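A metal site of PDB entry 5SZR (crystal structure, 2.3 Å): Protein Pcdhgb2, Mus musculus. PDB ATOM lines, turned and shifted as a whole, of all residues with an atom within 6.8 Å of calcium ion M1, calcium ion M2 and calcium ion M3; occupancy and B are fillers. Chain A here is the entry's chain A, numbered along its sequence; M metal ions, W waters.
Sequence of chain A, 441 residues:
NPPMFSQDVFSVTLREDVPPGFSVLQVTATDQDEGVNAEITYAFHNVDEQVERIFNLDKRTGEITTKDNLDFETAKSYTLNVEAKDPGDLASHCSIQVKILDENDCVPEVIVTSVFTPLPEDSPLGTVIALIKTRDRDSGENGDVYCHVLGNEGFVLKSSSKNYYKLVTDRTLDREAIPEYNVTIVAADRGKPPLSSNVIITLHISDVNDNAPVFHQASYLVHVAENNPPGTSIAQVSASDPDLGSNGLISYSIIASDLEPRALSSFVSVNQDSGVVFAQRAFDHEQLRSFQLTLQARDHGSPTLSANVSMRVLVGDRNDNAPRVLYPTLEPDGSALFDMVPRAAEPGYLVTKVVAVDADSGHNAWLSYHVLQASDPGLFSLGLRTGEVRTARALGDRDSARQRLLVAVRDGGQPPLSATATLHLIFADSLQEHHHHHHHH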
ATOM      1  N   GLU A  16      33.979   4.354   6.541  1.00  0.00           N
ATOM      2  CA  GLU A  16      33.362   3.164   7.115  1.00  0.00           C
ATOM      3  C   GLU A  16      32.562   2.344   6.102  1.00  0.00           C
ATOM      4  O   GLU A  16      32.195   1.208   6.407  1.00  0.00           O
ATOM      5  CB  GLU A  16      32.468   3.534   8.297  1.00  0.00           C
ATOM      6  CG  GLU A  16      31.322   4.479   7.965  1.00  0.00           C
ATOM      7  CD  GLU A  16      30.285   4.538   9.074  1.00  0.00           C
ATOM      8  OE1 GLU A  16      30.119   3.533   9.804  1.00  0.00           O
ATOM      9  OE2 GLU A  16      29.641   5.588   9.235  1.00  0.00           O
ATOM     10  N   LEU A  70      33.244  -2.443   7.715  1.00  0.00           N
ATOM     11  CA  LEU A  70      33.582  -1.532   8.790  1.00  0.00           C
ATOM     12  C   LEU A  70      32.317  -0.937   9.403  1.00  0.00           C
ATOM     13  O   LEU A  70      31.200  -1.140   8.907  1.00  0.00           O
ATOM     14  CB  LEU A  70      34.518  -0.434   8.288  1.00  0.00           C
ATOM     15  CG  LEU A  70      35.821  -0.926   7.630  1.00  0.00           C
ATOM     16  CD1 LEU A  70      36.729   0.226   7.214  1.00  0.00           C
ATOM     17  CD2 LEU A  70      36.555  -1.884   8.550  1.00  0.00           C
ATOM     18  N   ASP A  71      32.493  -0.220  10.509  1.00  0.00           N
ATOM     19  CA  ASP A  71      31.393   0.450  11.185  1.00  0.00           C
ATOM     20  C   ASP A  71      31.950   1.450  12.201  1.00  0.00           C
ATOM     21  O   ASP A  71      32.451   1.051  13.258  1.00  0.00           O
ATOM     22  CB  ASP A  71      30.468  -0.559  11.886  1.00  0.00           C
ATOM     23  CG  ASP A  71      29.320   0.094  12.624  1.00  0.00           C
ATOM     24  OD1 ASP A  71      28.991   1.259  12.327  1.00  0.00           O
ATOM     25  OD2 ASP A  71      28.729  -0.572  13.499  1.00  0.00           O
ATOM     26  N   PHE A  72      31.889   2.744  11.863  1.00  0.00           N
ATOM     27  CA  PHE A  72      32.428   3.784  12.738  1.00  0.00           C
ATOM     28  C   PHE A  72      31.751   3.767  14.099  1.00  0.00           C
ATOM     29  O   PHE A  72      32.378   4.096  15.105  1.00  0.00           O
ATOM     30  CB  PHE A  72      32.253   5.148  12.062  1.00  0.00           C
ATOM     31  CG  PHE A  72      32.719   6.306  12.895  1.00  0.00           C
ATOM     32  CD1 PHE A  72      34.037   6.722  12.849  1.00  0.00           C
ATOM     33  CD2 PHE A  72      31.831   6.993  13.725  1.00  0.00           C
ATOM     34  CE1 PHE A  72      34.467   7.795  13.603  1.00  0.00           C
ATOM     35  CE2 PHE A  72      32.261   8.066  14.479  1.00  0.00           C
ATOM     36  CZ  PHE A  72      33.587   8.474  14.424  1.00  0.00           C
ATOM     37  N   GLU A  73      30.469   3.392  14.151  1.00  0.00           N
ATOM     38  CA  GLU A  73      29.761   3.375  15.417  1.00  0.00           C
ATOM     39  C   GLU A  73      30.257   2.264  16.336  1.00  0.00           C
ATOM     40  O   GLU A  73      30.049   2.345  17.552  1.00  0.00           O
ATOM     41  CB  GLU A  73      28.251   3.227  15.164  1.00  0.00           C
ATOM     42  CG  GLU A  73      27.547   4.514  14.720  1.00  0.00           C
ATOM     43  CD  GLU A  73      28.094   5.094  13.413  1.00  0.00           C
ATOM     44  OE1 GLU A  73      28.255   4.335  12.440  1.00  0.00           O
ATOM     45  OE2 GLU A  73      28.355   6.316  13.378  1.00  0.00           O
ATOM     46  N   THR A  74      30.916   1.239  15.787  1.00  0.00           N
ATOM     47  CA  THR A  74      31.475   0.141  16.568  1.00  0.00           C
ATOM     48  C   THR A  74      32.953   0.328  16.893  1.00  0.00           C
ATOM     49  O   THR A  74      33.383   0.049  18.008  1.00  0.00           O
ATOM     50  CB  THR A  74      31.282  -1.190  15.819  1.00  0.00           C
ATOM     51  OG1 THR A  74      29.901  -1.384  15.515  1.00  0.00           O
ATOM     52  CG2 THR A  74      31.777  -2.353  16.659  1.00  0.00           C
ATOM     53  N   LEU A 101      36.534   6.907   9.238  1.00  0.00           N
ATOM     54  CA  LEU A 101      35.777   8.132   9.024  1.00  0.00           C
ATOM     55  C   LEU A 101      34.282   7.866   9.146  1.00  0.00           C
ATOM     56  O   LEU A 101      33.781   6.853   8.647  1.00  0.00           O
ATOM     57  CB  LEU A 101      36.095   8.742   7.653  1.00  0.00           C
ATOM     58  CG  LEU A 101      37.526   9.254   7.529  1.00  0.00           C
ATOM     59  CD1 LEU A 101      37.789   9.781   6.129  1.00  0.00           C
ATOM     60  CD2 LEU A 101      37.787  10.326   8.577  1.00  0.00           C
ATOM     61  N   ASP A 102      33.581   8.769   9.822  1.00  0.00           N
ATOM     62  CA  ASP A 102      32.158   8.614  10.042  1.00  0.00           C
ATOM     63  C   ASP A 102      31.373   8.992   8.783  1.00  0.00           C
ATOM     64  O   ASP A 102      31.573  10.070   8.219  1.00  0.00           O
ATOM     65  CB  ASP A 102      31.702   9.484  11.214  1.00  0.00           C
ATOM     66  CG  ASP A 102      30.200   9.614  11.305  1.00  0.00           C
ATOM     67  OD1 ASP A 102      29.502   8.589  11.163  1.00  0.00           O
ATOM     68  OD2 ASP A 102      29.706  10.746  11.510  1.00  0.00           O
ATOM     69  N   GLU A 103      30.496   8.093   8.355  1.00  0.00           N
ATOM     70  CA  GLU A 103      29.532   8.361   7.297  1.00  0.00           C
ATOM     71  C   GLU A 103      28.129   8.412   7.889  1.00  0.00           C
ATOM     72  O   GLU A 103      27.858   7.849   8.958  1.00  0.00           O
ATOM     73  CB  GLU A 103      29.589   7.280   6.205  1.00  0.00           C
ATOM     74  CG  GLU A 103      30.957   7.110   5.543  1.00  0.00           C
ATOM     75  CD  GLU A 103      31.342   8.294   4.675  1.00  0.00           C
ATOM     76  OE1 GLU A 103      32.527   8.701   4.724  1.00  0.00           O
ATOM     77  OE2 GLU A 103      30.468   8.813   3.964  1.00  0.00           O
ATOM     78  N   ASN A 104      27.245   9.095   7.172  1.00  0.00           N
ATOM     79  CA  ASN A 104      25.849   9.240   7.587  1.00  0.00           C
ATOM     80  C   ASN A 104      25.103   7.971   7.183  1.00  0.00           C
ATOM     81  O   ASN A 104      24.518   7.885   6.099  1.00  0.00           O
ATOM     82  CB  ASN A 104      25.235  10.487   6.963  1.00  0.00           C
ATOM     83  CG  ASN A 104      23.876  10.810   7.520  1.00  0.00           C
ATOM     84  OD1 ASN A 104      23.434  10.236   8.519  1.00  0.00           O
ATOM     85  ND2 ASN A 104      23.185  11.751   6.887  1.00  0.00           N
ATOM     86  N   ASP A 105      25.122   6.963   8.051  1.00  0.00           N
ATOM     87  CA  ASP A 105      24.431   5.715   7.786  1.00  0.00           C
ATOM     88  C   ASP A 105      23.473   5.308   8.903  1.00  0.00           C
ATOM     89  O   ASP A 105      22.994   4.171   8.900  1.00  0.00           O
ATOM     90  CB  ASP A 105      25.434   4.580   7.514  1.00  0.00           C
ATOM     91  CG  ASP A 105      26.380   4.337   8.670  1.00  0.00           C
ATOM     92  OD1 ASP A 105      26.504   5.201   9.548  1.00  0.00           O
ATOM     93  OD2 ASP A 105      27.021   3.263   8.684  1.00  0.00           O
ATOM     94  N   CYS A 106      23.182   6.203   9.847  1.00  0.00           N
ATOM     95  CA  CYS A 106      22.238   5.936  10.931  1.00  0.00           C
ATOM     96  C   CYS A 106      21.092   6.923  10.853  1.00  0.00           C
ATOM     97  O   CYS A 106      21.305   8.142  10.880  1.00  0.00           O
ATOM     98  CB  CYS A 106      22.928   6.021  12.295  1.00  0.00           C
ATOM     99  SG  CYS A 106      24.067   4.651  12.647  1.00  0.00           S
ATOM    100  N   VAL A 107      19.874   6.397  10.746  1.00  0.00           N
ATOM    101  CA  VAL A 107      18.669   7.230  10.596  1.00  0.00           C
ATOM    102  C   VAL A 107      18.360   7.896  11.938  1.00  0.00           C
ATOM    103  O   VAL A 107      18.607   7.295  12.989  1.00  0.00           O
ATOM    104  CB  VAL A 107      17.494   6.372  10.112  1.00  0.00           C
ATOM    105  CG1 VAL A 107      16.201   7.171  10.040  1.00  0.00           C
ATOM    106  CG2 VAL A 107      17.824   5.761   8.750  1.00  0.00           C
ATOM    107  N   PRO A 108      17.859   9.137  11.941  1.00  0.00           N
ATOM    108  CA  PRO A 108      17.348   9.701  13.200  1.00  0.00           C
ATOM    109  C   PRO A 108      16.089   8.972  13.649  1.00  0.00           C
ATOM    110  O   PRO A 108      15.272   8.549  12.833  1.00  0.00           O
ATOM    111  CB  PRO A 108      17.028  11.162  12.840  1.00  0.00           C
ATOM    112  CG  PRO A 108      17.737  11.419  11.542  1.00  0.00           C
ATOM    113  CD  PRO A 108      17.833  10.103  10.835  1.00  0.00           C
ATOM    114  N   ASP A 136      20.387   9.990  17.417  1.00  0.00           N
ATOM    115  CA  ASP A 136      21.051   9.719  16.142  1.00  0.00           C
ATOM    116  C   ASP A 136      22.424   9.140  16.447  1.00  0.00           C
ATOM    117  O   ASP A 136      23.256   9.820  17.062  1.00  0.00           O
ATOM    118  CB  ASP A 136      21.160  10.988  15.299  1.00  0.00           C
ATOM    119  CG  ASP A 136      21.524  10.691  13.847  1.00  0.00           C
ATOM    120  OD1 ASP A 136      22.546  10.009  13.596  1.00  0.00           O
ATOM    121  OD2 ASP A 136      20.765  11.126  12.951  1.00  0.00           O
ATOM    122  N   ARG A 137      22.662   7.907  16.012  1.00  0.00           N
ATOM    123  CA  ARG A 137      23.869   7.186  16.400  1.00  0.00           C
ATOM    124  C   ARG A 137      25.124   7.718  15.729  1.00  0.00           C
ATOM    125  O   ARG A 137      26.223   7.360  16.153  1.00  0.00           O
ATOM    126  CB  ARG A 137      23.691   5.701  16.077  1.00  0.00           C
ATOM    127  CG  ARG A 137      22.493   5.045  16.773  1.00  0.00           C
ATOM    128  CD  ARG A 137      22.533   3.541  16.596  1.00  0.00           C
ATOM    129  NE  ARG A 137      23.860   3.015  16.904  1.00  0.00           N
ATOM    130  CZ  ARG A 137      24.297   1.813  16.567  1.00  0.00           C
ATOM    131  NH1 ARG A 137      25.525   1.429  16.890  1.00  0.00           N
ATOM    132  NH2 ARG A 137      23.504   0.973  15.902  1.00  0.00           N
ATOM    133  N   ASP A 138      24.995   8.566  14.706  1.00  0.00           N
ATOM    134  CA  ASP A 138      26.140   9.149  14.030  1.00  0.00           C
ATOM    135  C   ASP A 138      26.744  10.275  14.853  1.00  0.00           C
ATOM    136  O   ASP A 138      26.176  10.738  15.851  1.00  0.00           O
ATOM    137  CB  ASP A 138      25.747   9.659  12.643  1.00  0.00           C
ATOM    138  CG  ASP A 138      25.380   8.547  11.685  1.00  0.00           C
ATOM    139  OD1 ASP A 138      25.955   7.446  11.824  1.00  0.00           O
ATOM    140  OD2 ASP A 138      24.524   8.763  10.800  1.00  0.00           O
ATOM    141  N   SER A 139      27.924  10.734  14.417  1.00  0.00           N
ATOM    142  CA  SER A 139      28.658  11.818  15.051  1.00  0.00           C
ATOM    143  C   SER A 139      28.535  13.097  14.226  1.00  0.00           C
ATOM    144  O   SER A 139      28.180  13.078  13.045  1.00  0.00           O
ATOM    145  CB  SER A 139      30.140  11.462  15.221  1.00  0.00           C
ATOM    146  OG  SER A 139      30.309  10.337  16.063  1.00  0.00           O
ATOM    147  N   GLU A 141      27.772  16.413  12.304  1.00  0.00           N
ATOM    148  CA  GLU A 141      26.599  16.875  11.569  1.00  0.00           C
ATOM    149  C   GLU A 141      25.675  15.719  11.204  1.00  0.00           C
ATOM    150  O   GLU A 141      24.453  15.882  11.158  1.00  0.00           O
ATOM    151  CB  GLU A 141      27.038  17.635  10.314  1.00  0.00           C
ATOM    152  CG  GLU A 141      27.721  18.955  10.609  1.00  0.00           C
ATOM    153  CD  GLU A 141      28.060  19.743   9.356  1.00  0.00           C
ATOM    154  OE1 GLU A 141      27.687  19.281   8.248  1.00  0.00           O
ATOM    155  OE2 GLU A 141      28.694  20.808   9.476  1.00  0.00           O
ATOM    156  N   ASN A 142      26.253  14.543  10.929  1.00  0.00           N
ATOM    157  CA  ASN A 142      25.431  13.388  10.607  1.00  0.00           C
ATOM    158  C   ASN A 142      24.513  12.993  11.758  1.00  0.00           C
ATOM    159  O   ASN A 142      23.458  12.388  11.535  1.00  0.00           O
ATOM    160  CB  ASN A 142      26.328  12.215  10.200  1.00  0.00           C
ATOM    161  CG  ASN A 142      27.211  12.547   9.007  1.00  0.00           C
ATOM    162  OD1 ASN A 142      27.136  13.645   8.448  1.00  0.00           O
ATOM    163  ND2 ASN A 142      28.057  11.598   8.617  1.00  0.00           N
ATOM    164  N   GLY A 143      24.884  13.338  12.990  1.00  0.00           N
ATOM    165  CA  GLY A 143      24.054  13.101  14.156  1.00  0.00           C
ATOM    166  C   GLY A 143      23.273  14.289  14.659  1.00  0.00           C
ATOM    167  O   GLY A 143      22.570  14.173  15.671  1.00  0.00           O
ATOM    168  N   ASP A 144      23.363  15.436  13.997  1.00  0.00           N
ATOM    169  CA  ASP A 144      22.642  16.632  14.399  1.00  0.00           C
ATOM    170  C   ASP A 144      21.252  16.594  13.783  1.00  0.00           C
ATOM    171  O   ASP A 144      21.106  16.737  12.561  1.00  0.00           O
ATOM    172  CB  ASP A 144      23.410  17.885  13.964  1.00  0.00           C
ATOM    173  CG  ASP A 144      23.155  19.061  14.883  1.00  0.00           C
ATOM    174  OD1 ASP A 144      23.167  18.879  16.115  1.00  0.00           O
ATOM    175  OD2 ASP A 144      22.960  20.190  14.373  1.00  0.00           O
ATOM    176  N   VAL A 145      20.229  16.426  14.623  1.00  0.00           N
ATOM    177  CA  VAL A 145      18.857  16.235  14.179  1.00  0.00           C
ATOM    178  C   VAL A 145      18.020  17.453  14.564  1.00  0.00           C
ATOM    179  O   VAL A 145      18.237  18.067  15.619  1.00  0.00           O
ATOM    180  CB  VAL A 145      18.245  14.946  14.767  1.00  0.00           C
ATOM    181  CG1 VAL A 145      16.850  14.697  14.199  1.00  0.00           C
ATOM    182  CG2 VAL A 145      19.145  13.770  14.512  1.00  0.00           C
ATOM    183  N   ASP A 189      18.514  14.581   9.796  1.00  0.00           N
ATOM    184  CA  ASP A 189      19.874  14.934  10.176  1.00  0.00           C
ATOM    185  C   ASP A 189      20.483  15.893   9.149  1.00  0.00           C
ATOM    186  O   ASP A 189      19.974  16.064   8.038  1.00  0.00           O
ATOM    187  CB  ASP A 189      20.760  13.684  10.331  1.00  0.00           C
ATOM    188  CG  ASP A 189      20.856  12.850   9.054  1.00  0.00           C
ATOM    189  OD1 ASP A 189      20.920  13.406   7.938  1.00  0.00           O
ATOM    190  OD2 ASP A 189      20.890  11.603   9.173  1.00  0.00           O
ATOM    191  N   ARG A 190      21.587  16.512   9.534  1.00  0.00           N
ATOM    192  CA  ARG A 190      22.254  17.485   8.668  1.00  0.00           C
ATOM    193  C   ARG A 190      23.553  16.918   8.105  1.00  0.00           C
ATOM    194  O   ARG A 190      24.595  17.582   8.120  1.00  0.00           O
ATOM    195  CB  ARG A 190      22.499  18.785   9.434  1.00  0.00           C
ATOM    196  CG  ARG A 190      21.210  19.476   9.863  1.00  0.00           C
ATOM    197  CD  ARG A 190      21.472  20.733  10.669  1.00  0.00           C
ATOM    198  NE  ARG A 190      20.240  21.445  10.983  1.00  0.00           N
ATOM    199  CZ  ARG A 190      19.891  22.620  10.458  1.00  0.00           C
ATOM    200  NH1 ARG A 190      20.693  23.221   9.586  1.00  0.00           N
ATOM    201  NH2 ARG A 190      18.748  23.192  10.803  1.00  0.00           N
ATOM    202  N   GLY A 191      23.495  15.690   7.593  1.00  0.00           N
ATOM    203  CA  GLY A 191      24.605  15.083   6.892  1.00  0.00           C
ATOM    204  C   GLY A 191      24.420  15.164   5.389  1.00  0.00           C
ATOM    205  O   GLY A 191      23.455  15.708   4.859  1.00  0.00           O
ATOM    206  N   LEU A 195      19.449  12.067   6.105  1.00  0.00           N
ATOM    207  CA  LEU A 195      18.486  11.015   6.387  1.00  0.00           C
ATOM    208  C   LEU A 195      17.398  11.548   7.294  1.00  0.00           C
ATOM    209  O   LEU A 195      17.636  12.417   8.131  1.00  0.00           O
ATOM    210  CB  LEU A 195      19.171   9.806   7.039  1.00  0.00           C
ATOM    211  CG  LEU A 195      20.255   9.098   6.215  1.00  0.00           C
ATOM    212  CD1 LEU A 195      20.960   8.041   7.041  1.00  0.00           C
ATOM    213  CD2 LEU A 195      19.643   8.486   4.968  1.00  0.00           C
HETATM  214 CA    CA M   1      27.923   2.692  10.782  1.00  0.00          CA
HETATM  215 CA    CA M   2      28.041   6.404  10.953  1.00  0.00          CA
HETATM  216 CA    CA M   3      22.469  10.299  10.838  1.00  0.00          CA
HETATM  217  O   HOH W   1      27.959   0.819   9.419  1.00  0.00           O
HETATM  218  O   HOH W   2      25.615   1.685  11.867  1.00  0.00           O
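Four residues have an atom within 4 Å of calcium ion M1: Glu 16, Asp 71, Glu 73 and Asp 105.
The nearest printed residue that does not touch calcium ion M1 is Phe 72 (4.1 Å).
Of the 27 residues printed, 6 come within 4 Å of calcium ion M2.
Calcium ion M1 is bound by water W1 (2.3 Å), OD2 of Asp 105 (2.4 Å), OE1 of Glu 73 (2.4 Å), OD1 of Asp 71 (2.4 Å), OE1 of Glu 16 (2.5 Å) and water W2 (2.7 Å).
Calcium ion M1 has six donor atoms within binding distance.
Slightly farther from calcium ion M1 lies OD1 of Asp 105 (3.1 Å).
The side-chain hydroxyl (OG1) of Thr 74 is in hydrogen-bond range of the side-chain carboxylate (OD2) of Asp 71, at 2.5 Å.
ND2 of Asn 142 lies within hydrogen-bond range of OD2 of Asp 102, 3.4 Å away.
OE1 of Glu 16 sits close to N of Phe 72, at 2.8 Å.
The backbone NH of Glu 16 sits at hydrogen-bond distance from the backbone carbonyl oxygen of Leu 101 (3.3 Å).
The side-chain carboxylate (OD2) of Asp 102 is in hydrogen-bond range of the backbone NH (N) of Ser 139.
The side-chain carboxylate (OD1) of Asp 189 sits at hydrogen-bond distance from the backbone NH (N) of Leu 195.
N of Gly 191 lies close to OD1 of Asp 189 (3.5 Å).
Six residues have an atom within 4 Å of calcium ion M3: Asn 104, Cys 106, Asp 136, Asp 138, Asn 142 and Asp 189.
The nearest printed residue that does not touch calcium ion M3 is Gly 143 (4.4 Å).
Calcium ion M3 is bound by O of Asn 142, O of Cys 106, OD1 of Asn 104, OD2 of Asp 138, OD2 of Asp 189, OD1 of Asp 136 and OD2 of Asp 136.
Calcium ion M3 has seven donor atoms within binding distance.
Calcium ion M2 is bound by the side-chain carboxylate (OD1) of Asp 105, 2.4 Å away.
Calcium ion M2 is bound by OE2 of Glu 73, at 2.4 Å.
Calcium ion M2 is bound by O of Glu 103.
OE2 of Glu 16 binds calcium ion M2 (2.5 Å).
OD1 of Asp 138 binds calcium ion M2 (2.5 Å).
OE1 of Glu 73 is bound to calcium ion M2.
Calcium ion M2 is bound by OD1 of Asp 102.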
